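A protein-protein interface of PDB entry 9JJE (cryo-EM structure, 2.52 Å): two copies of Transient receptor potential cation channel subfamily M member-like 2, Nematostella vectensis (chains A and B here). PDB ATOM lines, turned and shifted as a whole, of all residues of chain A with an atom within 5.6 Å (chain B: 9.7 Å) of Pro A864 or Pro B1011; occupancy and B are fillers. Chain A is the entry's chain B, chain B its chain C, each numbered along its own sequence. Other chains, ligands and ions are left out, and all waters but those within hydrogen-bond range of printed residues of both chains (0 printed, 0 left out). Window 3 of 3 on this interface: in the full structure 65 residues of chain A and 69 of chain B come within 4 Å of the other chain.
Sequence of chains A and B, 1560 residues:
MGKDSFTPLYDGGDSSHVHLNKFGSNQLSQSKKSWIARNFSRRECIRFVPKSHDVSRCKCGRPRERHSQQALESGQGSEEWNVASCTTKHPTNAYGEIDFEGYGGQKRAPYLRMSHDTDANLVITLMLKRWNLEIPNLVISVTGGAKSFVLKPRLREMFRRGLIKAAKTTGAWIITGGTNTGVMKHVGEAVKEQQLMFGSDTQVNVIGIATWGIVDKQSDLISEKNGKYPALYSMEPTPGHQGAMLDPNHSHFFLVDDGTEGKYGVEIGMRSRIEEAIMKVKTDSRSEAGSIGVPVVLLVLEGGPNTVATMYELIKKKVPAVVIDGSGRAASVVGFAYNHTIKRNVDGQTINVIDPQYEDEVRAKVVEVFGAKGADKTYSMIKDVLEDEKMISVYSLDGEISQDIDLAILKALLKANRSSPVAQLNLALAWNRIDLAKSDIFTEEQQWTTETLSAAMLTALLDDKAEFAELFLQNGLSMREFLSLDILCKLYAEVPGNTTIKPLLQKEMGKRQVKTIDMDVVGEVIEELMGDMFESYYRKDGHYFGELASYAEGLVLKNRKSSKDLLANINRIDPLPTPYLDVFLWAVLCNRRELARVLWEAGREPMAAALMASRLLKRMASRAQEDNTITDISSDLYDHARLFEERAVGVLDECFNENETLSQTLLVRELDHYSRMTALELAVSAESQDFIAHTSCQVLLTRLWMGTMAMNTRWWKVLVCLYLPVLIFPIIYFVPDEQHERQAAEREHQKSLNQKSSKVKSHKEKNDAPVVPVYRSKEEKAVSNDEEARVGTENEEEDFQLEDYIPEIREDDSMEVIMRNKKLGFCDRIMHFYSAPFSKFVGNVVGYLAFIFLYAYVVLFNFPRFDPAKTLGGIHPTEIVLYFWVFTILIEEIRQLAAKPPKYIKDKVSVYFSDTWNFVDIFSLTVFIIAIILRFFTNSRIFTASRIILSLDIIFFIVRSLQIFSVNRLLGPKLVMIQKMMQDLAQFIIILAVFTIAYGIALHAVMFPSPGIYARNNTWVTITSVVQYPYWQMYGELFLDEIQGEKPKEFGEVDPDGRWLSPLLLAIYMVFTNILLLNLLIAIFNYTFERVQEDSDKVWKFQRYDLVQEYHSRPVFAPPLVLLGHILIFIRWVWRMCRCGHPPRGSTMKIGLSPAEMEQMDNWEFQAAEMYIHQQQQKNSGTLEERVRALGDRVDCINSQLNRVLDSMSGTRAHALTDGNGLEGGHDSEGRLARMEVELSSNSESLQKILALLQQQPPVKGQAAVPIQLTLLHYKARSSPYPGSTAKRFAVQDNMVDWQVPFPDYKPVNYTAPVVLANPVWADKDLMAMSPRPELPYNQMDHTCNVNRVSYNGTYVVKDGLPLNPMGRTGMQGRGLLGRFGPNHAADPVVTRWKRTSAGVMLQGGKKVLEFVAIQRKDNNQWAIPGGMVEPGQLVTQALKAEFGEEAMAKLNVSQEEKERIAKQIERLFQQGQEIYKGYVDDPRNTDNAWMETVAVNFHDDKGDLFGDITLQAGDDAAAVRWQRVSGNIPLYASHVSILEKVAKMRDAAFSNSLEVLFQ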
ATOM      1  N   PHE A 861     -17.515 -13.905  -2.896  1.00  0.00           N
ATOM      2  CA  PHE A 861     -17.000 -14.044  -4.250  1.00  0.00           C
ATOM      3  C   PHE A 861     -16.066 -15.236  -4.427  1.00  0.00           C
ATOM      4  O   PHE A 861     -16.120 -15.909  -5.462  1.00  0.00           O
ATOM      5  CB  PHE A 861     -16.302 -12.754  -4.675  1.00  0.00           C
ATOM      6  CG  PHE A 861     -17.240 -11.604  -4.886  1.00  0.00           C
ATOM      7  CD1 PHE A 861     -17.969 -11.506  -6.060  1.00  0.00           C
ATOM      8  CD2 PHE A 861     -17.402 -10.630  -3.911  1.00  0.00           C
ATOM      9  CE1 PHE A 861     -18.842 -10.454  -6.263  1.00  0.00           C
ATOM     10  CE2 PHE A 861     -18.274  -9.572  -4.109  1.00  0.00           C
ATOM     11  CZ  PHE A 861     -18.995  -9.485  -5.287  1.00  0.00           C
ATOM     12  N   ASN A 862     -15.202 -15.516  -3.449  1.00  0.00           N
ATOM     13  CA  ASN A 862     -14.207 -16.566  -3.676  1.00  0.00           C
ATOM     14  C   ASN A 862     -13.849 -17.231  -2.341  1.00  0.00           C
ATOM     15  O   ASN A 862     -13.005 -16.737  -1.591  1.00  0.00           O
ATOM     16  CB  ASN A 862     -12.984 -15.993  -4.378  1.00  0.00           C
ATOM     17  CG  ASN A 862     -12.149 -17.055  -5.058  1.00  0.00           C
ATOM     18  OD1 ASN A 862     -12.391 -18.254  -4.906  1.00  0.00           O
ATOM     19  ND2 ASN A 862     -11.196 -16.616  -5.867  1.00  0.00           N
ATOM     20  N   PHE A 863     -14.505 -18.356  -2.066  1.00  0.00           N
ATOM     21  CA  PHE A 863     -14.155 -19.239  -0.950  1.00  0.00           C
ATOM     22  C   PHE A 863     -14.341 -20.672  -1.434  1.00  0.00           C
ATOM     23  O   PHE A 863     -15.347 -21.323  -1.130  1.00  0.00           O
ATOM     24  CB  PHE A 863     -15.015 -18.934   0.278  1.00  0.00           C
ATOM     25  CG  PHE A 863     -14.637 -19.708   1.504  1.00  0.00           C
ATOM     26  CD1 PHE A 863     -13.445 -19.445   2.160  1.00  0.00           C
ATOM     27  CD2 PHE A 863     -15.500 -20.652   2.039  1.00  0.00           C
ATOM     28  CE1 PHE A 863     -13.102 -20.142   3.298  1.00  0.00           C
ATOM     29  CE2 PHE A 863     -15.161 -21.347   3.183  1.00  0.00           C
ATOM     30  CZ  PHE A 863     -13.969 -21.088   3.815  1.00  0.00           C
ATOM     31  N   PRO A 864     -13.389 -21.194  -2.207  1.00  0.00           N
ATOM     32  CA  PRO A 864     -13.616 -22.454  -2.923  1.00  0.00           C
ATOM     33  C   PRO A 864     -13.456 -23.672  -2.026  1.00  0.00           C
ATOM     34  O   PRO A 864     -12.916 -23.604  -0.924  1.00  0.00           O
ATOM     35  CB  PRO A 864     -12.541 -22.432  -4.012  1.00  0.00           C
ATOM     36  CG  PRO A 864     -11.436 -21.661  -3.399  1.00  0.00           C
ATOM     37  CD  PRO A 864     -12.075 -20.612  -2.534  1.00  0.00           C
ATOM     38  N   ARG A 865     -13.944 -24.803  -2.528  1.00  0.00           N
ATOM     39  CA  ARG A 865     -13.777 -26.064  -1.820  1.00  0.00           C
ATOM     40  C   ARG A 865     -12.334 -26.535  -1.940  1.00  0.00           C
ATOM     41  O   ARG A 865     -11.735 -26.482  -3.018  1.00  0.00           O
ATOM     42  CB  ARG A 865     -14.738 -27.119  -2.371  1.00  0.00           C
ATOM     43  CG  ARG A 865     -14.758 -28.421  -1.584  1.00  0.00           C
ATOM     44  CD  ARG A 865     -15.831 -29.363  -2.105  1.00  0.00           C
ATOM     45  NE  ARG A 865     -15.858 -30.625  -1.372  1.00  0.00           N
ATOM     46  CZ  ARG A 865     -16.721 -31.608  -1.604  1.00  0.00           C
ATOM     47  NH1 ARG A 865     -17.639 -31.480  -2.554  1.00  0.00           N
ATOM     48  NH2 ARG A 865     -16.669 -32.721  -0.885  1.00  0.00           N
ATOM     49  N   PHE A 866     -11.775 -26.986  -0.818  1.00  0.00           N
ATOM     50  CA  PHE A 866     -10.377 -27.392  -0.780  1.00  0.00           C
ATOM     51  C   PHE A 866     -10.169 -28.690  -1.549  1.00  0.00           C
ATOM     52  O   PHE A 866     -10.963 -29.630  -1.443  1.00  0.00           O
ATOM     53  CB  PHE A 866      -9.913 -27.564   0.667  1.00  0.00           C
ATOM     54  CG  PHE A 866      -8.459 -27.926   0.804  1.00  0.00           C
ATOM     55  CD1 PHE A 866      -7.474 -26.970   0.614  1.00  0.00           C
ATOM     56  CD2 PHE A 866      -8.079 -29.219   1.138  1.00  0.00           C
ATOM     57  CE1 PHE A 866      -6.134 -27.296   0.745  1.00  0.00           C
ATOM     58  CE2 PHE A 866      -6.740 -29.553   1.269  1.00  0.00           C
ATOM     59  CZ  PHE A 866      -5.768 -28.588   1.073  1.00  0.00           C
ATOM     60  N   GLY A 874      -6.111 -24.675  -4.168  1.00  0.00           N
ATOM     61  CA  GLY A 874      -7.177 -23.891  -4.746  1.00  0.00           C
ATOM     62  C   GLY A 874      -7.465 -22.591  -4.034  1.00  0.00           C
ATOM     63  O   GLY A 874      -8.341 -21.842  -4.483  1.00  0.00           O
ATOM     64  N   ILE A 875      -6.748 -22.294  -2.948  1.00  0.00           N
ATOM     65  CA  ILE A 875      -7.034 -21.117  -2.138  1.00  0.00           C
ATOM     66  C   ILE A 875      -6.585 -19.865  -2.879  1.00  0.00           C
ATOM     67  O   ILE A 875      -5.443 -19.773  -3.345  1.00  0.00           O
ATOM     68  CB  ILE A 875      -6.341 -21.228  -0.771  1.00  0.00           C
ATOM     69  CG1 ILE A 875      -6.842 -22.455  -0.008  1.00  0.00           C
ATOM     70  CG2 ILE A 875      -6.584 -19.984   0.055  1.00  0.00           C
ATOM     71  CD1 ILE A 875      -6.020 -22.779   1.218  1.00  0.00           C
ATOM     72  N   HIS A 876      -7.494 -18.904  -3.011  1.00  0.00           N
ATOM     73  CA  HIS A 876      -7.150 -17.620  -3.593  1.00  0.00           C
ATOM     74  C   HIS A 876      -6.299 -16.830  -2.595  1.00  0.00           C
ATOM     75  O   HIS A 876      -6.491 -16.952  -1.382  1.00  0.00           O
ATOM     76  CB  HIS A 876      -8.428 -16.861  -3.954  1.00  0.00           C
ATOM     77  CG  HIS A 876      -8.212 -15.700  -4.873  1.00  0.00           C
ATOM     78  ND1 HIS A 876      -7.931 -14.432  -4.419  1.00  0.00           N
ATOM     79  CD2 HIS A 876      -8.196 -15.625  -6.224  1.00  0.00           C
ATOM     80  CE1 HIS A 876      -7.772 -13.622  -5.450  1.00  0.00           C
ATOM     81  NE2 HIS A 876      -7.929 -14.320  -6.558  1.00  0.00           N
ATOM     82  N   GLU A 879      -7.760 -14.923   0.368  1.00  0.00           N
ATOM     83  CA  GLU A 879      -8.002 -15.709   1.572  1.00  0.00           C
ATOM     84  C   GLU A 879      -6.726 -15.883   2.395  1.00  0.00           C
ATOM     85  O   GLU A 879      -6.790 -15.966   3.627  1.00  0.00           O
ATOM     86  CB  GLU A 879      -8.602 -17.062   1.177  1.00  0.00           C
ATOM     87  CG  GLU A 879      -9.004 -17.965   2.328  1.00  0.00           C
ATOM     88  CD  GLU A 879      -9.647 -19.259   1.865  1.00  0.00           C
ATOM     89  OE1 GLU A 879      -9.832 -19.436   0.642  1.00  0.00           O
ATOM     90  OE2 GLU A 879      -9.949 -20.110   2.727  1.00  0.00           O
ATOM     91  N   ARG A 935     -11.961 -25.791   7.060  1.00  0.00           N
ATOM     92  CA  ARG A 935     -11.626 -25.485   5.667  1.00  0.00           C
ATOM     93  C   ARG A 935     -11.054 -26.676   4.897  1.00  0.00           C
ATOM     94  O   ARG A 935     -11.433 -26.916   3.744  1.00  0.00           O
ATOM     95  CB  ARG A 935     -10.615 -24.336   5.651  1.00  0.00           C
ATOM     96  CG  ARG A 935     -10.091 -23.912   4.298  1.00  0.00           C
ATOM     97  CD  ARG A 935     -11.155 -23.175   3.544  1.00  0.00           C
ATOM     98  NE  ARG A 935     -10.668 -22.602   2.296  1.00  0.00           N
ATOM     99  CZ  ARG A 935     -10.680 -23.239   1.133  1.00  0.00           C
ATOM    100  NH1 ARG A 935     -11.172 -24.466   1.058  1.00  0.00           N
ATOM    101  NH2 ARG A 935     -10.225 -22.645   0.039  1.00  0.00           N
ATOM    102  N   PHE A 943     -17.013 -28.740   4.812  1.00  0.00           N
ATOM    103  CA  PHE A 943     -16.765 -27.466   4.140  1.00  0.00           C
ATOM    104  C   PHE A 943     -18.006 -26.581   4.124  1.00  0.00           C
ATOM    105  O   PHE A 943     -17.886 -25.346   4.165  1.00  0.00           O
ATOM    106  CB  PHE A 943     -16.261 -27.701   2.716  1.00  0.00           C
ATOM    107  CG  PHE A 943     -16.063 -26.438   1.940  1.00  0.00           C
ATOM    108  CD1 PHE A 943     -15.011 -25.589   2.235  1.00  0.00           C
ATOM    109  CD2 PHE A 943     -16.944 -26.089   0.926  1.00  0.00           C
ATOM    110  CE1 PHE A 943     -14.837 -24.417   1.531  1.00  0.00           C
ATOM    111  CE2 PHE A 943     -16.776 -24.918   0.216  1.00  0.00           C
ATOM    112  CZ  PHE A 943     -15.723 -24.080   0.522  1.00  0.00           C
ATOM    113  N   HIS B1004     -26.359 -13.336   1.689  1.00  0.00           N
ATOM    114  CA  HIS B1004     -25.977 -13.697   0.332  1.00  0.00           C
ATOM    115  C   HIS B1004     -24.838 -14.708   0.318  1.00  0.00           C
ATOM    116  O   HIS B1004     -24.714 -15.481  -0.638  1.00  0.00           O
ATOM    117  CB  HIS B1004     -25.583 -12.461  -0.473  1.00  0.00           C
ATOM    118  CG  HIS B1004     -25.401 -12.742  -1.931  1.00  0.00           C
ATOM    119  ND1 HIS B1004     -24.224 -13.232  -2.453  1.00  0.00           N
ATOM    120  CD2 HIS B1004     -26.257 -12.628  -2.974  1.00  0.00           C
ATOM    121  CE1 HIS B1004     -24.359 -13.402  -3.756  1.00  0.00           C
ATOM    122  NE2 HIS B1004     -25.581 -13.038  -4.098  1.00  0.00           N
ATOM    123  N   ALA B1005     -24.005 -14.730   1.361  1.00  0.00           N
ATOM    124  CA  ALA B1005     -22.943 -15.720   1.403  1.00  0.00           C
ATOM    125  C   ALA B1005     -23.472 -17.103   1.765  1.00  0.00           C
ATOM    126  O   ALA B1005     -22.905 -18.109   1.326  1.00  0.00           O
ATOM    127  CB  ALA B1005     -21.863 -15.268   2.381  1.00  0.00           C
ATOM    128  N   PHE B1008     -25.908 -18.087  -1.670  1.00  0.00           N
ATOM    129  CA  PHE B1008     -25.244 -18.215  -2.965  1.00  0.00           C
ATOM    130  C   PHE B1008     -23.739 -18.350  -2.757  1.00  0.00           C
ATOM    131  O   PHE B1008     -23.005 -17.351  -2.822  1.00  0.00           O
ATOM    132  CB  PHE B1008     -25.570 -17.013  -3.856  1.00  0.00           C
ATOM    133  CG  PHE B1008     -27.019 -16.925  -4.267  1.00  0.00           C
ATOM    134  CD1 PHE B1008     -27.487 -17.638  -5.356  1.00  0.00           C
ATOM    135  CD2 PHE B1008     -27.909 -16.119  -3.567  1.00  0.00           C
ATOM    136  CE1 PHE B1008     -28.817 -17.553  -5.748  1.00  0.00           C
ATOM    137  CE2 PHE B1008     -29.245 -16.030  -3.947  1.00  0.00           C
ATOM    138  CZ  PHE B1008     -29.697 -16.750  -5.037  1.00  0.00           C
ATOM    139  N   PRO B1009     -23.246 -19.564  -2.483  1.00  0.00           N
ATOM    140  CA  PRO B1009     -21.793 -19.783  -2.455  1.00  0.00           C
ATOM    141  C   PRO B1009     -21.195 -19.579  -3.839  1.00  0.00           C
ATOM    142  O   PRO B1009     -21.584 -20.239  -4.804  1.00  0.00           O
ATOM    143  CB  PRO B1009     -21.658 -21.242  -2.000  1.00  0.00           C
ATOM    144  CG  PRO B1009     -22.950 -21.572  -1.341  1.00  0.00           C
ATOM    145  CD  PRO B1009     -23.979 -20.785  -2.101  1.00  0.00           C
ATOM    146  N   SER B1010     -20.259 -18.638  -3.936  1.00  0.00           N
ATOM    147  CA  SER B1010     -19.793 -18.204  -5.253  1.00  0.00           C
ATOM    148  C   SER B1010     -18.795 -19.149  -5.925  1.00  0.00           C
ATOM    149  O   SER B1010     -18.642 -19.061  -7.156  1.00  0.00           O
ATOM    150  CB  SER B1010     -19.246 -16.782  -5.166  1.00  0.00           C
ATOM    151  OG  SER B1010     -18.716 -16.367  -6.414  1.00  0.00           O
ATOM    152  N   PRO B1011     -17.999 -19.956  -5.217  1.00  0.00           N
ATOM    153  CA  PRO B1011     -17.410 -21.083  -5.982  1.00  0.00           C
ATOM    154  C   PRO B1011     -18.227 -22.367  -5.868  1.00  0.00           C
ATOM    155  O   PRO B1011     -17.865 -23.331  -5.177  1.00  0.00           O
ATOM    156  CB  PRO B1011     -16.020 -21.217  -5.363  1.00  0.00           C
ATOM    157  CG  PRO B1011     -15.771 -19.940  -4.679  1.00  0.00           C
ATOM    158  CD  PRO B1011     -17.091 -19.522  -4.144  1.00  0.00           C
ATOM    159  N   GLY B1012     -19.364 -22.391  -6.556  1.00  0.00           N
ATOM    160  CA  GLY B1012     -20.240 -23.548  -6.532  1.00  0.00           C
ATOM    161  C   GLY B1012     -21.258 -23.473  -7.647  1.00  0.00           C
ATOM    162  O   GLY B1012     -21.265 -22.543  -8.456  1.00  0.00           O
ATOM    163  N   ILE B1013     -22.120 -24.495  -7.695  1.00  0.00           N
ATOM    164  CA  ILE B1013     -23.214 -24.503  -8.661  1.00  0.00           C
ATOM    165  C   ILE B1013     -24.269 -23.455  -8.328  1.00  0.00           C
ATOM    166  O   ILE B1013     -25.021 -23.033  -9.211  1.00  0.00           O
ATOM    167  CB  ILE B1013     -23.844 -25.911  -8.770  1.00  0.00           C
ATOM    168  CG1 ILE B1013     -24.449 -26.357  -7.443  1.00  0.00           C
ATOM    169  CG2 ILE B1013     -22.809 -26.924  -9.208  1.00  0.00           C
ATOM    170  CD1 ILE B1013     -25.304 -27.596  -7.557  1.00  0.00           C
ATOM    171  N   TYR B1014     -24.342 -23.020  -7.072  1.00  0.00           N
ATOM    172  CA  TYR B1014     -25.282 -21.991  -6.643  1.00  0.00           C
ATOM    173  C   TYR B1014     -24.694 -20.591  -6.709  1.00  0.00           C
ATOM    174  O   TYR B1014     -25.152 -19.702  -5.985  1.00  0.00           O
ATOM    175  CB  TYR B1014     -25.771 -22.283  -5.227  1.00  0.00           C
ATOM    176  CG  TYR B1014     -26.556 -23.563  -5.156  1.00  0.00           C
ATOM    177  CD1 TYR B1014     -27.874 -23.611  -5.585  1.00  0.00           C
ATOM    178  CD2 TYR B1014     -25.977 -24.729  -4.676  1.00  0.00           C
ATOM    179  CE1 TYR B1014     -28.599 -24.777  -5.538  1.00  0.00           C
ATOM    180  CE2 TYR B1014     -26.692 -25.906  -4.630  1.00  0.00           C
ATOM    181  CZ  TYR B1014     -28.004 -25.923  -5.060  1.00  0.00           C
ATOM    182  OH  TYR B1014     -28.733 -27.089  -5.011  1.00  0.00           O
ATOM    183  N   ALA B1015     -23.668 -20.390  -7.529  1.00  0.00           N
ATOM    184  CA  ALA B1015     -22.994 -19.105  -7.622  1.00  0.00           C
ATOM    185  C   ALA B1015     -23.799 -18.114  -8.443  1.00  0.00           C
ATOM    186  O   ALA B1015     -24.162 -18.395  -9.584  1.00  0.00           O
ATOM    187  CB  ALA B1015     -21.626 -19.288  -8.266  1.00  0.00           C
ATOM    188  N   ARG B1016     -24.039 -16.933  -7.884  1.00  0.00           N
ATOM    189  CA  ARG B1016     -24.367 -15.802  -8.738  1.00  0.00           C
ATOM    190  C   ARG B1016     -23.094 -15.302  -9.404  1.00  0.00           C
ATOM    191  O   ARG B1016     -22.208 -14.753  -8.740  1.00  0.00           O
ATOM    192  CB  ARG B1016     -25.050 -14.695  -7.949  1.00  0.00           C
ATOM    193  CG  ARG B1016     -26.494 -15.021  -7.627  1.00  0.00           C
ATOM    194  CD  ARG B1016     -27.193 -13.858  -6.953  1.00  0.00           C
ATOM    195  NE  ARG B1016     -28.604 -14.143  -6.719  1.00  0.00           N
ATOM    196  CZ  ARG B1016     -29.438 -13.316  -6.100  1.00  0.00           C
ATOM    197  NH1 ARG B1016     -29.006 -12.152  -5.644  1.00  0.00           N
ATOM    198  NH2 ARG B1016     -30.706 -13.659  -5.929  1.00  0.00           N
ATOM    199  N   ASN B1017     -23.006 -15.496 -10.718  1.00  0.00           N
ATOM    200  CA  ASN B1017     -21.796 -15.198 -11.483  1.00  0.00           C
ATOM    201  C   ASN B1017     -21.860 -13.774 -12.037  1.00  0.00           C
ATOM    202  O   ASN B1017     -21.764 -13.518 -13.237  1.00  0.00           O
ATOM    203  CB  ASN B1017     -21.623 -16.234 -12.586  1.00  0.00           C
ATOM    204  CG  ASN B1017     -21.298 -17.605 -12.031  1.00  0.00           C
ATOM    205  OD1 ASN B1017     -20.410 -17.749 -11.190  1.00  0.00           O
ATOM    206  ND2 ASN B1017     -22.035 -18.615 -12.472  1.00  0.00           N
ATOM    207  N   ASP B1055     -28.716 -22.333  -2.274  1.00  0.00           N
ATOM    208  CA  ASP B1055     -28.061 -23.512  -1.721  1.00  0.00           C
ATOM    209  C   ASP B1055     -28.960 -24.167  -0.671  1.00  0.00           C
ATOM    210  O   ASP B1055     -29.579 -23.459   0.132  1.00  0.00           O
ATOM    211  CB  ASP B1055     -26.720 -23.119  -1.099  1.00  0.00           C
ATOM    212  CG  ASP B1055     -25.923 -24.312  -0.613  1.00  0.00           C
ATOM    213  OD1 ASP B1055     -25.372 -25.044  -1.460  1.00  0.00           O
ATOM    214  OD2 ASP B1055     -25.848 -24.516   0.618  1.00  0.00           O
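The backbone carbonyl oxygen (O) of Phe A861 sits at hydrogen-bond distance from the side-chain hydroxyl (OG) of Ser B1010 (2.8 Å).
NH1 of Arg A935 sits at hydrogen-bond distance from O of Pro A864 (2.8 Å).
Pro B1011 touches Phe A861.
Asn A862 touches Pro B1011.
Phe A863 touches Pro B1011.
Pro A864 touches Pro B1011 (CA to CB, 3.6 Å).
Of the printed residues of chain B, Phe A861 touches Ser B1010 and Pro B1011.
Phe A863 touches one residue of chain B.
His A876 touches none of the printed residues of chain B.
Arg A935 touches none of the printed residues of chain B.
Of the printed residues of chain A, Ser B1010 touches Phe A861 (2.8 Å).
Pro B1011 touches just these residues of chain A: Phe A861 (3.97 Å), Asn A862 (3.8 Å), Phe A863 (3.3 Å) and Pro A864 (3.6 Å).
The nearest residue of chain B that does not touch Pro A864 is Gly B1012 (6.8 Å).
Hydrophobic or aromatic side chains of chain A within 4 Å of the printed part of chain B: Pro A864.
Hydrophobic or aromatic side chains of chain B that line the printed part of chain A: Pro B1011.
Among the printed residues, 5 pairs touch across the chains.
Among the printed residues, no Asp or Glu carboxylate lies within 4 Å of a Lys or Arg side-chain nitrogen of the other chain.
No position is printed for both chains.
Of the 5 pairs that touch across the chains among the printed residues, none has its exchanged pair printed and touching as well.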
